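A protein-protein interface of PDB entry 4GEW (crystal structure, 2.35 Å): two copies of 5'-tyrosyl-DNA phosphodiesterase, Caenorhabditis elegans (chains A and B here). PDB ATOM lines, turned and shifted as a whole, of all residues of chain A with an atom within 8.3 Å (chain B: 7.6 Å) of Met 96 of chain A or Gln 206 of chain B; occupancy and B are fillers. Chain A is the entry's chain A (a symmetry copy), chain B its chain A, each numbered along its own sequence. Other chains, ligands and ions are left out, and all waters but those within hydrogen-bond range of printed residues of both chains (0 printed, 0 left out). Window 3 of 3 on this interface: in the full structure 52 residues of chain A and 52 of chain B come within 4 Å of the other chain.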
ATOM      1  N   GLU A  89      11.647 -27.997   5.029  1.00  0.00           N
ATOM      2  CA  GLU A  89      13.041 -27.658   4.768  1.00  0.00           C
ATOM      3  C   GLU A  89      13.681 -28.685   3.841  1.00  0.00           C
ATOM      4  O   GLU A  89      14.437 -28.332   2.936  1.00  0.00           O
ATOM      5  CB  GLU A  89      13.830 -27.561   6.074  1.00  0.00           C
ATOM      6  CG  GLU A  89      13.401 -26.413   6.976  1.00  0.00           C
ATOM      7  CD  GLU A  89      13.746 -25.047   6.401  1.00  0.00           C
ATOM      8  OE1 GLU A  89      14.830 -24.520   6.737  1.00  0.00           O
ATOM      9  OE2 GLU A  89      12.932 -24.501   5.621  1.00  0.00           O
ATOM     10  N   ALA A  90      13.367 -29.957   4.072  1.00  0.00           N
ATOM     11  CA  ALA A  90      13.911 -31.040   3.264  1.00  0.00           C
ATOM     12  C   ALA A  90      13.417 -30.946   1.827  1.00  0.00           C
ATOM     13  O   ALA A  90      14.171 -31.179   0.885  1.00  0.00           O
ATOM     14  CB  ALA A  90      13.547 -32.391   3.868  1.00  0.00           C
ATOM     15  N   ARG A  91      12.147 -30.597   1.662  1.00  0.00           N
ATOM     16  CA  ARG A  91      11.582 -30.440   0.329  1.00  0.00           C
ATOM     17  C   ARG A  91      12.174 -29.221  -0.378  1.00  0.00           C
ATOM     18  O   ARG A  91      12.395 -29.237  -1.588  1.00  0.00           O
ATOM     19  CB  ARG A  91      10.057 -30.348   0.394  1.00  0.00           C
ATOM     20  CG  ARG A  91       9.379 -31.665   0.748  1.00  0.00           C
ATOM     21  CD  ARG A  91       7.865 -31.579   0.599  1.00  0.00           C
ATOM     22  NE  ARG A  91       7.273 -30.659   1.566  1.00  0.00           N
ATOM     23  CZ  ARG A  91       6.949 -30.992   2.811  1.00  0.00           C
ATOM     24  NH1 ARG A  91       7.158 -32.227   3.247  1.00  0.00           N
ATOM     25  NH2 ARG A  91       6.417 -30.089   3.623  1.00  0.00           N
ATOM     26  N   SER A  92      12.436 -28.166   0.385  1.00  0.00           N
ATOM     27  CA  SER A  92      13.029 -26.960  -0.170  1.00  0.00           C
ATOM     28  C   SER A  92      14.451 -27.242  -0.638  1.00  0.00           C
ATOM     29  O   SER A  92      14.880 -26.743  -1.678  1.00  0.00           O
ATOM     30  CB  SER A  92      13.015 -25.830   0.863  1.00  0.00           C
ATOM     31  OG  SER A  92      13.636 -24.668   0.342  1.00  0.00           O
ATOM     32  N   ALA A  93      15.173 -28.057   0.126  1.00  0.00           N
ATOM     33  CA  ALA A  93      16.522 -28.471  -0.247  1.00  0.00           C
ATOM     34  C   ALA A  93      16.505 -29.378  -1.478  1.00  0.00           C
ATOM     35  O   ALA A  93      17.404 -29.326  -2.314  1.00  0.00           O
ATOM     36  CB  ALA A  93      17.202 -29.174   0.919  1.00  0.00           C
ATOM     37  N   ALA A  94      15.477 -30.211  -1.587  1.00  0.00           N
ATOM     38  CA  ALA A  94      15.391 -31.156  -2.691  1.00  0.00           C
ATOM     39  C   ALA A  94      15.020 -30.454  -3.994  1.00  0.00           C
ATOM     40  O   ALA A  94      15.445 -30.861  -5.074  1.00  0.00           O
ATOM     41  CB  ALA A  94      14.391 -32.259  -2.371  1.00  0.00           C
ATOM     42  N   VAL A  95      14.224 -29.397  -3.891  1.00  0.00           N
ATOM     43  CA  VAL A  95      13.775 -28.671  -5.073  1.00  0.00           C
ATOM     44  C   VAL A  95      14.707 -27.510  -5.407  1.00  0.00           C
ATOM     45  O   VAL A  95      15.056 -27.303  -6.568  1.00  0.00           O
ATOM     46  CB  VAL A  95      12.325 -28.159  -4.903  1.00  0.00           C
ATOM     47  CG1 VAL A  95      11.913 -27.283  -6.080  1.00  0.00           C
ATOM     48  CG2 VAL A  95      11.370 -29.332  -4.752  1.00  0.00           C
ATOM     49  N   MET A  96      15.129 -26.774  -4.383  1.00  0.00           N
ATOM     50  CA  MET A  96      15.918 -25.558  -4.579  1.00  0.00           C
ATOM     51  C   MET A  96      17.394 -25.671  -4.187  1.00  0.00           C
ATOM     52  O   MET A  96      18.221 -24.891  -4.656  1.00  0.00           O
ATOM     53  CB  MET A  96      15.279 -24.395  -3.822  1.00  0.00           C
ATOM     54  CG  MET A  96      13.896 -24.061  -4.314  1.00  0.00           C
ATOM     55  SD  MET A  96      13.920 -23.717  -6.078  1.00  0.00           S
ATOM     56  CE  MET A  96      15.062 -22.334  -6.133  1.00  0.00           C
ATOM     57  N   GLY A  97      17.718 -26.626  -3.325  1.00  0.00           N
ATOM     58  CA  GLY A  97      19.078 -26.765  -2.835  1.00  0.00           C
ATOM     59  C   GLY A  97      19.372 -25.805  -1.700  1.00  0.00           C
ATOM     60  O   GLY A  97      20.465 -25.242  -1.621  1.00  0.00           O
ATOM     61  N   VAL B 202       8.979 -15.320  -9.836  1.00  0.00           N
ATOM     62  CA  VAL B 202       9.186 -16.590 -10.508  1.00  0.00           C
ATOM     63  C   VAL B 202      10.273 -17.369  -9.787  1.00  0.00           C
ATOM     64  O   VAL B 202      11.399 -16.899  -9.653  1.00  0.00           O
ATOM     65  CB  VAL B 202       9.589 -16.400 -11.982  1.00  0.00           C
ATOM     66  CG1 VAL B 202       9.799 -17.758 -12.652  1.00  0.00           C
ATOM     67  CG2 VAL B 202       8.538 -15.582 -12.725  1.00  0.00           C
ATOM     68  N   ILE B 203       9.923 -18.558  -9.314  1.00  0.00           N
ATOM     69  CA  ILE B 203      10.877 -19.437  -8.660  1.00  0.00           C
ATOM     70  C   ILE B 203      11.281 -20.548  -9.618  1.00  0.00           C
ATOM     71  O   ILE B 203      10.434 -21.296 -10.095  1.00  0.00           O
ATOM     72  CB  ILE B 203      10.269 -20.067  -7.393  1.00  0.00           C
ATOM     73  CG1 ILE B 203       9.850 -18.970  -6.406  1.00  0.00           C
ATOM     74  CG2 ILE B 203      11.254 -21.039  -6.752  1.00  0.00           C
ATOM     75  CD1 ILE B 203       9.166 -19.489  -5.163  1.00  0.00           C
ATOM     76  N   HIS B 204      12.572 -20.654  -9.905  1.00  0.00           N
ATOM     77  CA  HIS B 204      13.056 -21.696 -10.804  1.00  0.00           C
ATOM     78  C   HIS B 204      13.391 -22.965 -10.029  1.00  0.00           C
ATOM     79  O   HIS B 204      14.259 -22.951  -9.161  1.00  0.00           O
ATOM     80  CB  HIS B 204      14.287 -21.209 -11.574  1.00  0.00           C
ATOM     81  CG  HIS B 204      14.036 -19.978 -12.390  1.00  0.00           C
ATOM     82  ND1 HIS B 204      13.920 -20.006 -13.763  1.00  0.00           N
ATOM     83  CD2 HIS B 204      13.870 -18.686 -12.025  1.00  0.00           C
ATOM     84  CE1 HIS B 204      13.697 -18.784 -14.209  1.00  0.00           C
ATOM     85  NE2 HIS B 204      13.661 -17.963 -13.175  1.00  0.00           N
ATOM     86  N   PHE B 205      12.694 -24.056 -10.340  1.00  0.00           N
ATOM     87  CA  PHE B 205      12.974 -25.348  -9.720  1.00  0.00           C
ATOM     88  C   PHE B 205      14.383 -25.808 -10.080  1.00  0.00           C
ATOM     89  O   PHE B 205      14.695 -26.002 -11.256  1.00  0.00           O
ATOM     90  CB  PHE B 205      11.963 -26.401 -10.190  1.00  0.00           C
ATOM     91  CG  PHE B 205      10.530 -26.074  -9.853  1.00  0.00           C
ATOM     92  CD1 PHE B 205      10.214 -25.378  -8.699  1.00  0.00           C
ATOM     93  CD2 PHE B 205       9.499 -26.478 -10.692  1.00  0.00           C
ATOM     94  CE1 PHE B 205       8.891 -25.083  -8.387  1.00  0.00           C
ATOM     95  CE2 PHE B 205       8.178 -26.190 -10.387  1.00  0.00           C
ATOM     96  CZ  PHE B 205       7.874 -25.491  -9.231  1.00  0.00           C
ATOM     97  N   GLN B 206      15.233 -25.989  -9.074  1.00  0.00           N
ATOM     98  CA  GLN B 206      16.617 -26.390  -9.320  1.00  0.00           C
ATOM     99  C   GLN B 206      16.762 -27.867  -9.646  1.00  0.00           C
ATOM    100  O   GLN B 206      17.788 -28.285 -10.168  1.00  0.00           O
ATOM    101  CB  GLN B 206      17.521 -26.026  -8.141  1.00  0.00           C
ATOM    102  CG  GLN B 206      17.659 -24.531  -7.922  1.00  0.00           C
ATOM    103  CD  GLN B 206      18.111 -23.797  -9.172  1.00  0.00           C
ATOM    104  OE1 GLN B 206      19.107 -24.164  -9.798  1.00  0.00           O
ATOM    105  NE2 GLN B 206      17.374 -22.755  -9.544  1.00  0.00           N
ATOM    106  N   ASN B 207      15.746 -28.660  -9.330  1.00  0.00           N
ATOM    107  CA  ASN B 207      15.788 -30.080  -9.660  1.00  0.00           C
ATOM    108  C   ASN B 207      15.163 -30.363 -11.024  1.00  0.00           C
ATOM    109  O   ASN B 207      14.962 -31.514 -11.399  1.00  0.00           O
ATOM    110  CB  ASN B 207      15.114 -30.918  -8.568  1.00  0.00           C
ATOM    111  CG  ASN B 207      13.606 -30.745  -8.539  1.00  0.00           C
ATOM    112  OD1 ASN B 207      13.067 -29.753  -9.036  1.00  0.00           O
ATOM    113  ND2 ASN B 207      12.916 -31.712  -7.947  1.00  0.00           N
ATOM    114  N   SER B 208      14.851 -29.302 -11.762  1.00  0.00           N
ATOM    115  CA  SER B 208      14.213 -29.450 -13.063  1.00  0.00           C
ATOM    116  C   SER B 208      15.221 -29.409 -14.208  1.00  0.00           C
ATOM    117  O   SER B 208      16.090 -28.535 -14.254  1.00  0.00           O
ATOM    118  CB  SER B 208      13.156 -28.370 -13.272  1.00  0.00           C
ATOM    119  OG  SER B 208      12.559 -28.490 -14.553  1.00  0.00           O
ATOM    120  N   GLY B 209      15.096 -30.361 -15.127  1.00  0.00           N
ATOM    121  CA  GLY B 209      15.884 -30.360 -16.346  1.00  0.00           C
ATOM    122  C   GLY B 209      15.045 -29.856 -17.507  1.00  0.00           C
ATOM    123  O   GLY B 209      15.419 -30.023 -18.666  1.00  0.00           O
ATOM    124  N   ARG B 212      11.347 -25.754 -15.578  1.00  0.00           N
ATOM    125  CA  ARG B 212      10.069 -25.547 -14.900  1.00  0.00           C
ATOM    126  C   ARG B 212      10.191 -24.581 -13.723  1.00  0.00           C
ATOM    127  O   ARG B 212      11.230 -24.510 -13.063  1.00  0.00           O
ATOM    128  CB  ARG B 212       9.450 -26.882 -14.487  1.00  0.00           C
ATOM    129  CG  ARG B 212       9.401 -27.875 -15.651  1.00  0.00           C
ATOM    130  CD  ARG B 212       8.694 -27.253 -16.857  1.00  0.00           C
ATOM    131  NE  ARG B 212       8.743 -28.126 -18.021  1.00  0.00           N
ATOM    132  CZ  ARG B 212       7.961 -29.187 -18.182  1.00  0.00           C
ATOM    133  NH1 ARG B 212       7.069 -29.496 -17.245  1.00  0.00           N
ATOM    134  NH2 ARG B 212       8.077 -29.940 -19.269  1.00  0.00           N
ATOM    135  N   GLN B 242      11.067 -35.886  -9.282  1.00  0.00           N
ATOM    136  CA  GLN B 242      11.157 -34.438  -9.415  1.00  0.00           C
ATOM    137  C   GLN B 242       9.785 -33.796  -9.281  1.00  0.00           C
ATOM    138  O   GLN B 242       9.619 -32.799  -8.579  1.00  0.00           O
ATOM    139  CB  GLN B 242      11.791 -34.053 -10.755  1.00  0.00           C
ATOM    140  CG  GLN B 242      13.276 -34.385 -10.869  1.00  0.00           C
ATOM    141  CD  GLN B 242      13.529 -35.855 -11.117  1.00  0.00           C
ATOM    142  OE1 GLN B 242      12.922 -36.461 -12.000  1.00  0.00           O
ATOM    143  NE2 GLN B 242      14.424 -36.442 -10.332  1.00  0.00           N
ATOM    144  N   GLN B 246       8.535 -31.222  -6.354  1.00  0.00           N
ATOM    145  CA  GLN B 246       7.998 -29.924  -6.776  1.00  0.00           C
ATOM    146  C   GLN B 246       6.587 -29.662  -6.229  1.00  0.00           C
ATOM    147  O   GLN B 246       6.302 -28.587  -5.696  1.00  0.00           O
ATOM    148  CB  GLN B 246       8.007 -29.813  -8.307  1.00  0.00           C
ATOM    149  CG  GLN B 246       9.404 -29.694  -8.910  1.00  0.00           C
ATOM    150  CD  GLN B 246       9.430 -29.962 -10.408  1.00  0.00           C
ATOM    151  OE1 GLN B 246       8.389 -30.166 -11.040  1.00  0.00           O
ATOM    152  NE2 GLN B 246      10.631 -29.972 -10.983  1.00  0.00           N
ATOM    153  N   PHE B 249       6.591 -28.933  -2.555  1.00  0.00           N
ATOM    154  CA  PHE B 249       7.205 -27.627  -2.383  1.00  0.00           C
ATOM    155  C   PHE B 249       6.181 -26.532  -2.680  1.00  0.00           C
ATOM    156  O   PHE B 249       6.051 -25.566  -1.931  1.00  0.00           O
ATOM    157  CB  PHE B 249       8.417 -27.503  -3.310  1.00  0.00           C
ATOM    158  CG  PHE B 249       9.044 -26.137  -3.327  1.00  0.00           C
ATOM    159  CD1 PHE B 249       9.900 -25.736  -2.313  1.00  0.00           C
ATOM    160  CD2 PHE B 249       8.795 -25.259  -4.377  1.00  0.00           C
ATOM    161  CE1 PHE B 249      10.492 -24.476  -2.336  1.00  0.00           C
ATOM    162  CE2 PHE B 249       9.381 -23.999  -4.412  1.00  0.00           C
ATOM    163  CZ  PHE B 249      10.231 -23.607  -3.389  1.00  0.00           C
ATOM    164  N   LYS B 253       4.400 -23.586  -0.240  1.00  0.00           N
ATOM    165  CA  LYS B 253       4.238 -22.166  -0.546  1.00  0.00           C
ATOM    166  C   LYS B 253       2.793 -21.722  -0.357  1.00  0.00           C
ATOM    167  O   LYS B 253       2.534 -20.661   0.214  1.00  0.00           O
ATOM    168  CB  LYS B 253       4.723 -21.870  -1.968  1.00  0.00           C
ATOM    169  CG  LYS B 253       6.173 -21.381  -2.052  1.00  0.00           C
ATOM    170  CD  LYS B 253       7.109 -22.176  -1.142  1.00  0.00           C
ATOM    171  CE  LYS B 253       8.292 -21.335  -0.664  1.00  0.00           C
ATOM    172  NZ  LYS B 253       9.084 -22.047   0.391  1.00  0.00           N
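The backbone carbonyl oxygen (O) of Val 95 of chain A sits at hydrogen-bond distance from the backbone NH (N) of Gln 206 of chain B (2.8 Å).
O of Val 95 of chain A lies within hydrogen-bond range of N of Asn 207 of chain B, at 3.2 Å.
SD of Met 96 of chain A lies close to O of His 204 of chain B, at 3.2 Å.
The backbone carbonyl oxygen (O) of Ser 92 of chain A lies within hydrogen-bond range of the backbone NH (N) of Gly 97 of chain A (3.3 Å).
NE2 of Gln 206 of chain B lies within hydrogen-bond range of O of His 204 of chain B (3.1 Å).
The backbone NH (N) of Phe 205 of chain B sits at hydrogen-bond distance from the backbone carbonyl oxygen (O) of Arg 212 of chain B, at 3.1 Å.
OD1 of Asn 207 of chain B sits at hydrogen-bond distance from NE2 of Gln 246 of chain B (3.1 Å).
CA of Ser 92 of chain A touches CD1 of Phe 249 of chain B (3.99 Å).
O of Ala 94 of chain A touches CB of Asn 207 of chain B, 3.5 Å away.
CD1 of Phe 205 of chain B touches CG1 of Val 95 of chain A, at 3.7 Å.
N of Gln 246 of chain B touches CG2 of Val 95 of chain A, at 3.8 Å.
Phe 249 of chain B touches Val 95 of chain A (CB to CG2, 3.8 Å).
SD of Met 96 of chain A touches CG2 of Ile 203 of chain B, 3.8 Å away.
CG of Gln 206 of chain B touches O of Met 96 of chain A, at 3.3 Å.
Phe 249 of chain B touches Met 96 of chain A.
Met 96 of chain A touches just these residues of chain B: Ile 203, His 204, Gln 206 and Phe 249.
Gln 206 of chain B touches two residues of chain A.
Printed residues of chain A within 4 Å of Phe 249 of chain B: Ser 92 (3.99 Å), Val 95 (3.8 Å) and Met 96 (3.8 Å).
Printed residues of chain A within 4 Å of Ile 203 of chain B: Met 96.
Of the printed residues of chain A, Phe 205 of chain B touches Val 95 (3.7 Å).
Printed residues of chain A that touch a printed residue of chain B: Ser 92, Ala 94, Val 95 and Met 96.
Hydrophobic or aromatic side chains of chain A within 4 Å of the printed part of chain B: Val 95 and Met 96.
Among the printed residues, 11 pairs touch across the chains.
Among the printed residues, no Asp or Glu carboxylate lies within 4 Å of a Lys or Arg side-chain nitrogen of the other chain.
No position is printed for both chains.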
